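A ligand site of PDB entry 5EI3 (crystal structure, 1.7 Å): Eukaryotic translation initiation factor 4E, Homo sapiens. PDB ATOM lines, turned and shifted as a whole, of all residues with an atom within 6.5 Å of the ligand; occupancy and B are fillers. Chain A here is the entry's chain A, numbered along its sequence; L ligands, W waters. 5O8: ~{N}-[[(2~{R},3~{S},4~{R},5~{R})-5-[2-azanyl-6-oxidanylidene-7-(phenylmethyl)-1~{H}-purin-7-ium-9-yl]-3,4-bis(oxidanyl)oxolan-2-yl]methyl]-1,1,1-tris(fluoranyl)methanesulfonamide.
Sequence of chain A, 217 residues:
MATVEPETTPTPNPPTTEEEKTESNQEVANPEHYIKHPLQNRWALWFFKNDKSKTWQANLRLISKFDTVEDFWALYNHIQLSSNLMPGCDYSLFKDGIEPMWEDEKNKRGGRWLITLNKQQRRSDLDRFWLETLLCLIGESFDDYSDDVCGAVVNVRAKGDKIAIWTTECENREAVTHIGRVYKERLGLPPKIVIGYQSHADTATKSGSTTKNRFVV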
ATOM      1  N   PHE A  48     -25.034   4.392  -0.014  1.00  0.00           N
ATOM      2  CA  PHE A  48     -25.827   3.398   0.695  1.00  0.00           C
ATOM      3  C   PHE A  48     -25.845   3.771   2.172  1.00  0.00           C
ATOM      4  O   PHE A  48     -24.793   3.882   2.790  1.00  0.00           O
ATOM      5  CB  PHE A  48     -25.271   1.987   0.507  1.00  0.00           C
ATOM      6  CG  PHE A  48     -26.040   0.938   1.252  1.00  0.00           C
ATOM      7  CD1 PHE A  48     -27.160   0.348   0.682  1.00  0.00           C
ATOM      8  CD2 PHE A  48     -25.666   0.558   2.533  1.00  0.00           C
ATOM      9  CE1 PHE A  48     -27.879  -0.607   1.382  1.00  0.00           C
ATOM     10  CE2 PHE A  48     -26.378  -0.390   3.230  1.00  0.00           C
ATOM     11  CZ  PHE A  48     -27.485  -0.979   2.654  1.00  0.00           C
ATOM     12  N   THR A  55     -35.176  -2.100   3.053  1.00  0.00           N
ATOM     13  CA  THR A  55     -34.466  -3.100   2.248  1.00  0.00           C
ATOM     14  C   THR A  55     -33.152  -2.521   1.718  1.00  0.00           C
ATOM     15  O   THR A  55     -32.960  -1.302   1.666  1.00  0.00           O
ATOM     16  CB  THR A  55     -35.307  -3.556   1.062  1.00  0.00           C
ATOM     17  OG1 THR A  55     -35.632  -2.436   0.229  1.00  0.00           O
ATOM     18  CG2 THR A  55     -36.590  -4.245   1.528  1.00  0.00           C
ATOM     19  N   TRP A  56     -32.265  -3.424   1.311  1.00  0.00           N
ATOM     20  CA  TRP A  56     -30.973  -2.999   0.772  1.00  0.00           C
ATOM     21  C   TRP A  56     -31.165  -2.063  -0.423  1.00  0.00           C
ATOM     22  O   TRP A  56     -30.530  -1.017  -0.517  1.00  0.00           O
ATOM     23  CB  TRP A  56     -30.135  -4.213   0.369  1.00  0.00           C
ATOM     24  CG  TRP A  56     -28.736  -3.889  -0.081  1.00  0.00           C
ATOM     25  CD1 TRP A  56     -27.637  -3.715   0.724  1.00  0.00           C
ATOM     26  CD2 TRP A  56     -28.278  -3.697  -1.430  1.00  0.00           C
ATOM     27  NE1 TRP A  56     -26.533  -3.432  -0.045  1.00  0.00           N
ATOM     28  CE2 TRP A  56     -26.894  -3.412  -1.371  1.00  0.00           C
ATOM     29  CE3 TRP A  56     -28.907  -3.733  -2.675  1.00  0.00           C
ATOM     30  CZ2 TRP A  56     -26.134  -3.168  -2.515  1.00  0.00           C
ATOM     31  CZ3 TRP A  56     -28.154  -3.496  -3.816  1.00  0.00           C
ATOM     32  CH2 TRP A  56     -26.776  -3.221  -3.721  1.00  0.00           C
ATOM     33  N   GLN A  57     -32.077  -2.438  -1.326  1.00  0.00           N
ATOM     34  CA  GLN A  57     -32.301  -1.667  -2.549  1.00  0.00           C
ATOM     35  C   GLN A  57     -32.818  -0.265  -2.235  1.00  0.00           C
ATOM     36  O   GLN A  57     -32.416   0.718  -2.875  1.00  0.00           O
ATOM     37  CB  GLN A  57     -33.276  -2.415  -3.460  1.00  0.00           C
ATOM     38  CG  GLN A  57     -32.773  -3.750  -4.073  1.00  0.00           C
ATOM     39  CD  GLN A  57     -33.822  -4.492  -4.924  1.00  0.00           C
ATOM     40  OE1 GLN A  57     -35.032  -4.309  -4.725  1.00  0.00           O
ATOM     41  NE2 GLN A  57     -33.351  -5.343  -5.849  1.00  0.00           N
ATOM     42  N   ASP A  90     -21.937   2.703   2.344  1.00  0.00           N
ATOM     43  CA  ASP A  90     -21.157   2.470   1.125  1.00  0.00           C
ATOM     44  C   ASP A  90     -21.105   3.732   0.270  1.00  0.00           C
ATOM     45  O   ASP A  90     -22.025   4.555   0.311  1.00  0.00           O
ATOM     46  CB  ASP A  90     -21.831   1.385   0.254  1.00  0.00           C
ATOM     47  CG  ASP A  90     -21.878   0.016   0.901  1.00  0.00           C
ATOM     48  OD1 ASP A  90     -21.115  -0.204   1.864  1.00  0.00           O
ATOM     49  OD2 ASP A  90     -22.660  -0.834   0.442  1.00  0.00           O
ATOM     50  N   PRO A 100     -25.392  -0.075  -9.246  1.00  0.00           N
ATOM     51  CA  PRO A 100     -24.370  -0.699  -8.389  1.00  0.00           C
ATOM     52  C   PRO A 100     -24.891  -1.909  -7.619  1.00  0.00           C
ATOM     53  O   PRO A 100     -24.755  -1.990  -6.393  1.00  0.00           O
ATOM     54  CB  PRO A 100     -23.968   0.453  -7.463  1.00  0.00           C
ATOM     55  CG  PRO A 100     -25.192   1.321  -7.400  1.00  0.00           C
ATOM     56  CD  PRO A 100     -25.916   1.189  -8.689  1.00  0.00           C
ATOM     57  N   MET A 101     -25.483  -2.850  -8.343  1.00  0.00           N
ATOM     58  CA  MET A 101     -26.016  -4.074  -7.772  1.00  0.00           C
ATOM     59  C   MET A 101     -25.726  -5.209  -8.736  1.00  0.00           C
ATOM     60  O   MET A 101     -25.708  -5.017  -9.956  1.00  0.00           O
ATOM     61  CB  MET A 101     -27.536  -3.951  -7.494  1.00  0.00           C
ATOM     62  CG  MET A 101     -28.389  -3.767  -8.733  1.00  0.00           C
ATOM     63  SD  MET A 101     -30.147  -3.546  -8.300  1.00  0.00           S
ATOM     64  CE  MET A 101     -30.062  -2.084  -7.288  1.00  0.00           C
ATOM     65  N   TRP A 102     -25.472  -6.406  -8.204  1.00  0.00           N
ATOM     66  CA  TRP A 102     -24.970  -7.466  -9.060  1.00  0.00           C
ATOM     67  C   TRP A 102     -26.026  -7.958 -10.043  1.00  0.00           C
ATOM     68  O   TRP A 102     -25.668  -8.520 -11.074  1.00  0.00           O
ATOM     69  CB  TRP A 102     -24.388  -8.622  -8.236  1.00  0.00           C
ATOM     70  CG  TRP A 102     -25.368  -9.673  -7.757  1.00  0.00           C
ATOM     71  CD1 TRP A 102     -26.094  -9.652  -6.583  1.00  0.00           C
ATOM     72  CD2 TRP A 102     -25.689 -10.909  -8.408  1.00  0.00           C
ATOM     73  NE1 TRP A 102     -26.860 -10.803  -6.494  1.00  0.00           N
ATOM     74  CE2 TRP A 102     -26.626 -11.585  -7.595  1.00  0.00           C
ATOM     75  CE3 TRP A 102     -25.274 -11.500  -9.607  1.00  0.00           C
ATOM     76  CZ2 TRP A 102     -27.162 -12.825  -7.948  1.00  0.00           C
ATOM     77  CZ3 TRP A 102     -25.806 -12.741  -9.951  1.00  0.00           C
ATOM     78  CH2 TRP A 102     -26.732 -13.391  -9.117  1.00  0.00           C
ATOM     79  N   GLU A 103     -27.302  -7.695  -9.754  1.00  0.00           N
ATOM     80  CA  GLU A 103     -28.367  -8.115 -10.677  1.00  0.00           C
ATOM     81  C   GLU A 103     -28.394  -7.320 -11.984  1.00  0.00           C
ATOM     82  O   GLU A 103     -29.048  -7.777 -12.936  1.00  0.00           O
ATOM     83  CB  GLU A 103     -29.706  -7.986  -9.959  1.00  0.00           C
ATOM     84  CG  GLU A 103     -29.813  -8.884  -8.746  1.00  0.00           C
ATOM     85  CD  GLU A 103     -29.621  -8.152  -7.425  1.00  0.00           C
ATOM     86  OE1 GLU A 103     -28.782  -7.230  -7.345  1.00  0.00           O
ATOM     87  OE2 GLU A 103     -30.309  -8.520  -6.435  1.00  0.00           O
ATOM     88  N   ARG A 112     -15.784  -9.237  -8.719  1.00  0.00           N
ATOM     89  CA  ARG A 112     -15.056  -8.087  -8.170  1.00  0.00           C
ATOM     90  C   ARG A 112     -13.678  -8.485  -7.650  1.00  0.00           C
ATOM     91  O   ARG A 112     -13.506  -9.555  -7.060  1.00  0.00           O
ATOM     92  CB  ARG A 112     -15.856  -7.431  -7.030  1.00  0.00           C
ATOM     93  CG  ARG A 112     -16.140  -8.376  -5.870  1.00  0.00           C
ATOM     94  CD  ARG A 112     -17.038  -7.763  -4.799  1.00  0.00           C
ATOM     95  NE  ARG A 112     -17.290  -8.755  -3.763  1.00  0.00           N
ATOM     96  CZ  ARG A 112     -17.566  -8.473  -2.484  1.00  0.00           C
ATOM     97  NH1 ARG A 112     -17.657  -7.207  -2.075  1.00  0.00           N
ATOM     98  NH2 ARG A 112     -17.768  -9.457  -1.618  1.00  0.00           N
ATOM     99  N   ASN A 155     -16.966  -0.227   1.169  1.00  0.00           N
ATOM    100  CA  ASN A 155     -17.804  -0.580   2.314  1.00  0.00           C
ATOM    101  C   ASN A 155     -17.117  -0.130   3.587  1.00  0.00           C
ATOM    102  O   ASN A 155     -16.016  -0.594   3.887  1.00  0.00           O
ATOM    103  CB  ASN A 155     -18.026  -2.101   2.408  1.00  0.00           C
ATOM    104  CG  ASN A 155     -18.443  -2.750   1.109  1.00  0.00           C
ATOM    105  OD1 ASN A 155     -17.748  -3.639   0.619  1.00  0.00           O
ATOM    106  ND2 ASN A 155     -19.604  -2.365   0.580  1.00  0.00           N
ATOM    107  N   TRP A 166     -15.516  -3.745  -9.621  1.00  0.00           N
ATOM    108  CA  TRP A 166     -16.430  -4.688 -10.262  1.00  0.00           C
ATOM    109  C   TRP A 166     -16.177  -4.724 -11.766  1.00  0.00           C
ATOM    110  O   TRP A 166     -16.057  -3.667 -12.402  1.00  0.00           O
ATOM    111  CB  TRP A 166     -17.882  -4.268 -10.012  1.00  0.00           C
ATOM    112  CG  TRP A 166     -18.382  -4.408  -8.589  1.00  0.00           C
ATOM    113  CD1 TRP A 166     -17.655  -4.340  -7.434  1.00  0.00           C
ATOM    114  CD2 TRP A 166     -19.738  -4.664  -8.197  1.00  0.00           C
ATOM    115  NE1 TRP A 166     -18.491  -4.525  -6.334  1.00  0.00           N
ATOM    116  CE2 TRP A 166     -19.763  -4.740  -6.788  1.00  0.00           C
ATOM    117  CE3 TRP A 166     -20.927  -4.849  -8.913  1.00  0.00           C
ATOM    118  CZ2 TRP A 166     -20.939  -4.985  -6.068  1.00  0.00           C
ATOM    119  CZ3 TRP A 166     -22.094  -5.078  -8.207  1.00  0.00           C
ATOM    120  CH2 TRP A 166     -22.095  -5.149  -6.798  1.00  0.00           C
ATOM    121  N   SER A 199     -16.549 -14.108  -8.081  1.00  0.00           N
ATOM    122  CA  SER A 199     -17.714 -14.037  -8.944  1.00  0.00           C
ATOM    123  C   SER A 199     -18.967 -13.674  -8.136  1.00  0.00           C
ATOM    124  O   SER A 199     -19.162 -14.177  -7.027  1.00  0.00           O
ATOM    125  CB  SER A 199     -17.908 -15.384  -9.639  1.00  0.00           C
ATOM    126  OG  SER A 199     -19.273 -15.692  -9.756  1.00  0.00           O
ATOM    127  N   HIS A 200     -19.804 -12.793  -8.690  1.00  0.00           N
ATOM    128  CA  HIS A 200     -21.029 -12.421  -7.985  1.00  0.00           C
ATOM    129  C   HIS A 200     -21.963 -13.623  -7.853  1.00  0.00           C
ATOM    130  O   HIS A 200     -22.604 -13.814  -6.807  1.00  0.00           O
ATOM    131  CB  HIS A 200     -21.761 -11.286  -8.715  1.00  0.00           C
ATOM    132  CG  HIS A 200     -20.975 -10.009  -8.796  1.00  0.00           C
ATOM    133  ND1 HIS A 200     -20.321  -9.451  -7.718  1.00  0.00           N
ATOM    134  CD2 HIS A 200     -20.797  -9.148  -9.836  1.00  0.00           C
ATOM    135  CE1 HIS A 200     -19.747  -8.314  -8.095  1.00  0.00           C
ATOM    136  NE2 HIS A 200     -20.025  -8.113  -9.370  1.00  0.00           N
ATOM    137  N   ALA A 201     -22.072 -14.431  -8.911  1.00  0.00           N
ATOM    138  CA  ALA A 201     -22.921 -15.615  -8.864  1.00  0.00           C
ATOM    139  C   ALA A 201     -22.431 -16.604  -7.814  1.00  0.00           C
ATOM    140  O   ALA A 201     -23.247 -17.219  -7.110  1.00  0.00           O
ATOM    141  CB  ALA A 201     -22.993 -16.269 -10.246  1.00  0.00           C
ATOM    142  N   ASP A 202     -21.110 -16.785  -7.697  1.00  0.00           N
ATOM    143  CA  ASP A 202     -20.559 -17.623  -6.623  1.00  0.00           C
ATOM    144  C   ASP A 202     -20.951 -17.081  -5.251  1.00  0.00           C
ATOM    145  O   ASP A 202     -21.344 -17.842  -4.360  1.00  0.00           O
ATOM    146  CB  ASP A 202     -19.033 -17.688  -6.716  1.00  0.00           C
ATOM    147  CG  ASP A 202     -18.540 -18.538  -7.865  1.00  0.00           C
ATOM    148  OD1 ASP A 202     -19.376 -19.137  -8.578  1.00  0.00           O
ATOM    149  OD2 ASP A 202     -17.306 -18.624  -8.052  1.00  0.00           O
ATOM    150  N   THR A 203     -20.814 -15.765  -5.049  1.00  0.00           N
ATOM    151  CA  THR A 203     -21.206 -15.170  -3.772  1.00  0.00           C
ATOM    152  C   THR A 203     -22.689 -15.399  -3.493  1.00  0.00           C
ATOM    153  O   THR A 203     -23.076 -15.693  -2.361  1.00  0.00           O
ATOM    154  CB  THR A 203     -20.877 -13.680  -3.776  1.00  0.00           C
ATOM    155  OG1 THR A 203     -19.477 -13.511  -4.045  1.00  0.00           O
ATOM    156  CG2 THR A 203     -21.226 -13.022  -2.444  1.00  0.00           C
ATOM    157  N   ALA A 204     -23.514 -15.301  -4.531  1.00  0.00           N
ATOM    158  CA  ALA A 204     -24.954 -15.408  -4.358  1.00  0.00           C
ATOM    159  C   ALA A 204     -25.416 -16.838  -4.099  1.00  0.00           C
ATOM    160  O   ALA A 204     -26.555 -17.036  -3.638  1.00  0.00           O
ATOM    161  CB  ALA A 204     -25.674 -14.848  -5.589  1.00  0.00           C
ATOM    162  N   THR A 205     -24.586 -17.844  -4.379  1.00  0.00           N
ATOM    163  CA  THR A 205     -25.013 -19.237  -4.290  1.00  0.00           C
ATOM    164  C   THR A 205     -24.213 -20.081  -3.318  1.00  0.00           C
ATOM    165  O   THR A 205     -24.585 -21.230  -3.076  1.00  0.00           O
ATOM    166  CB  THR A 205     -24.975 -19.913  -5.673  1.00  0.00           C
ATOM    167  OG1 THR A 205     -23.641 -19.846  -6.215  1.00  0.00           O
ATOM    168  CG2 THR A 205     -25.954 -19.237  -6.635  1.00  0.00           C
ATOM    169  N   LYS A 206     -23.127 -19.560  -2.752  1.00  0.00           N
ATOM    170  CA  LYS A 206     -22.232 -20.373  -1.924  1.00  0.00           C
ATOM    171  C   LYS A 206     -22.952 -20.894  -0.681  1.00  0.00           C
ATOM    172  O   LYS A 206     -23.840 -20.241  -0.127  1.00  0.00           O
ATOM    173  CB  LYS A 206     -21.019 -19.553  -1.504  1.00  0.00           C
ATOM    174  CG  LYS A 206     -21.383 -18.461  -0.498  1.00  0.00           C
ATOM    175  CD  LYS A 206     -20.165 -17.665  -0.051  1.00  0.00           C
ATOM    176  CE  LYS A 206     -20.574 -16.319   0.528  1.00  0.00           C
ATOM    177  NZ  LYS A 206     -21.289 -16.453   1.822  1.00  0.00           N
HETATM  178  C4  5O8 L   1     -26.972  -6.948  -1.917  1.00  0.00           C
HETATM  179  C5  5O8 L   1     -26.125  -6.578  -2.951  1.00  0.00           C
HETATM  180  C6  5O8 L   1     -26.561  -6.597  -4.268  1.00  0.00           C
HETATM  181  C8  5O8 L   1     -25.056  -6.417  -1.065  1.00  0.00           C
HETATM  182  N1  5O8 L   1     -27.871  -6.994  -4.525  1.00  0.00           N
HETATM  183  N2  5O8 L   1     -29.943  -7.744  -3.675  1.00  0.00           N
HETATM  184  N3  5O8 L   1     -28.226  -7.332  -2.189  1.00  0.00           N
HETATM  185  CAM 5O8 L   1     -21.925  -7.417  -2.421  1.00  0.00           C
HETATM  186  CAK 5O8 L   1     -21.133  -8.531  -2.664  1.00  0.00           C
HETATM  187  CAJ 5O8 L   1     -21.303  -9.273  -3.829  1.00  0.00           C
HETATM  188  CAL 5O8 L   1     -22.269  -8.901  -4.760  1.00  0.00           C
HETATM  189  CAN 5O8 L   1     -23.061  -7.773  -4.516  1.00  0.00           C
HETATM  190  CAW 5O8 L   1     -22.898  -7.037  -3.348  1.00  0.00           C
HETATM  191  CAQ 5O8 L   1     -23.771  -5.812  -3.095  1.00  0.00           C
HETATM  192  N7  5O8 L   1     -24.974  -6.262  -2.378  1.00  0.00           N
HETATM  193  O6  5O8 L   1     -25.818  -6.269  -5.177  1.00  0.00           O
HETATM  194  C2  5O8 L   1     -28.688  -7.362  -3.449  1.00  0.00           C
HETATM  195  N9  5O8 L   1     -26.279  -6.840  -0.784  1.00  0.00           N
HETATM  196  CBD 5O8 L   1     -26.762  -7.127   0.599  1.00  0.00           C
HETATM  197  OAU 5O8 L   1     -26.080  -8.341   1.039  1.00  0.00           O
HETATM  198  CBB 5O8 L   1     -28.242  -7.328   0.756  1.00  0.00           C
HETATM  199  OAF 5O8 L   1     -28.617  -7.004   2.090  1.00  0.00           O
HETATM  200  CBA 5O8 L   1     -28.351  -8.837   0.537  1.00  0.00           C
HETATM  201  OAE 5O8 L   1     -29.382  -9.325   1.377  1.00  0.00           O
HETATM  202  CBC 5O8 L   1     -27.030  -9.438   1.058  1.00  0.00           C
HETATM  203  CAP 5O8 L   1     -26.521 -10.647   0.200  1.00  0.00           C
HETATM  204  NAS 5O8 L   1     -26.985 -10.436  -1.194  1.00  0.00           N
HETATM  205  SBH 5O8 L   1     -25.772 -10.322  -2.311  1.00  0.00           S
HETATM  206  OAC 5O8 L   1     -24.566  -9.672  -1.697  1.00  0.00           O
HETATM  207  OAD 5O8 L   1     -26.245  -9.506  -3.483  1.00  0.00           O
HETATM  208  CBG 5O8 L   1     -25.365 -12.014  -2.857  1.00  0.00           C
HETATM  209  FAH 5O8 L   1     -24.946 -12.721  -1.812  1.00  0.00           F
HETATM  210  FAI 5O8 L   1     -26.444 -12.583  -3.377  1.00  0.00           F
HETATM  211  FAG 5O8 L   1     -24.404 -11.957  -3.767  1.00  0.00           F
HETATM  212  O   HOH W   1     -29.050 -12.037  -4.842  1.00  0.00           O
HETATM  213  O   HOH W   2     -29.534 -11.214  -2.294  1.00  0.00           O
HETATM  214  O   HOH W   3     -30.956  -6.877   3.147  1.00  0.00           O
HETATM  215  O   HOH W   4     -29.335  -9.974   3.988  1.00  0.00           O
HETATM  216  O   HOH W   5     -23.046  -9.796   0.670  1.00  0.00           O
HETATM  217  O   HOH W   6     -31.951  -9.161  -1.621  1.00  0.00           O
HETATM  218  O   HOH W   7     -27.404  -4.682   4.347  1.00  0.00           O
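N2 of the ligand sits at hydrogen-bond distance from OE2 of Glu 103 (2.9 Å).
The backbone NH (N) of Trp 102 sits at hydrogen-bond distance from an oxygen (O6) of the ligand (3.0 Å).
The indole nitrogen (NE1) of Trp 102 sits close to an oxygen (OAD) of the ligand (3.3 Å).
The backbone carbonyl oxygen of Ser 199 sits at hydrogen-bond distance from the side-chain hydroxyl of Thr 203 (3.1 Å).
The indole nitrogen of Trp 56 lies close to a nitrogen (N9) of the ligand (3.5 Å).
Merely in contact with the ligand: Ala 204 (3.3 Å), Met 101 (3.4 Å), Thr 203 (3.6 Å), Arg 112 (3.6 Å), His 200 (3.6 Å) and Trp 166 (3.6 Å).
Hydrophobic or aromatic side chains that line the ligand: Trp 56, Met 101, Trp 102, Trp 166 and Ala 204.
Of the 20 residues printed, 9 come within 4 Å of the ligand.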
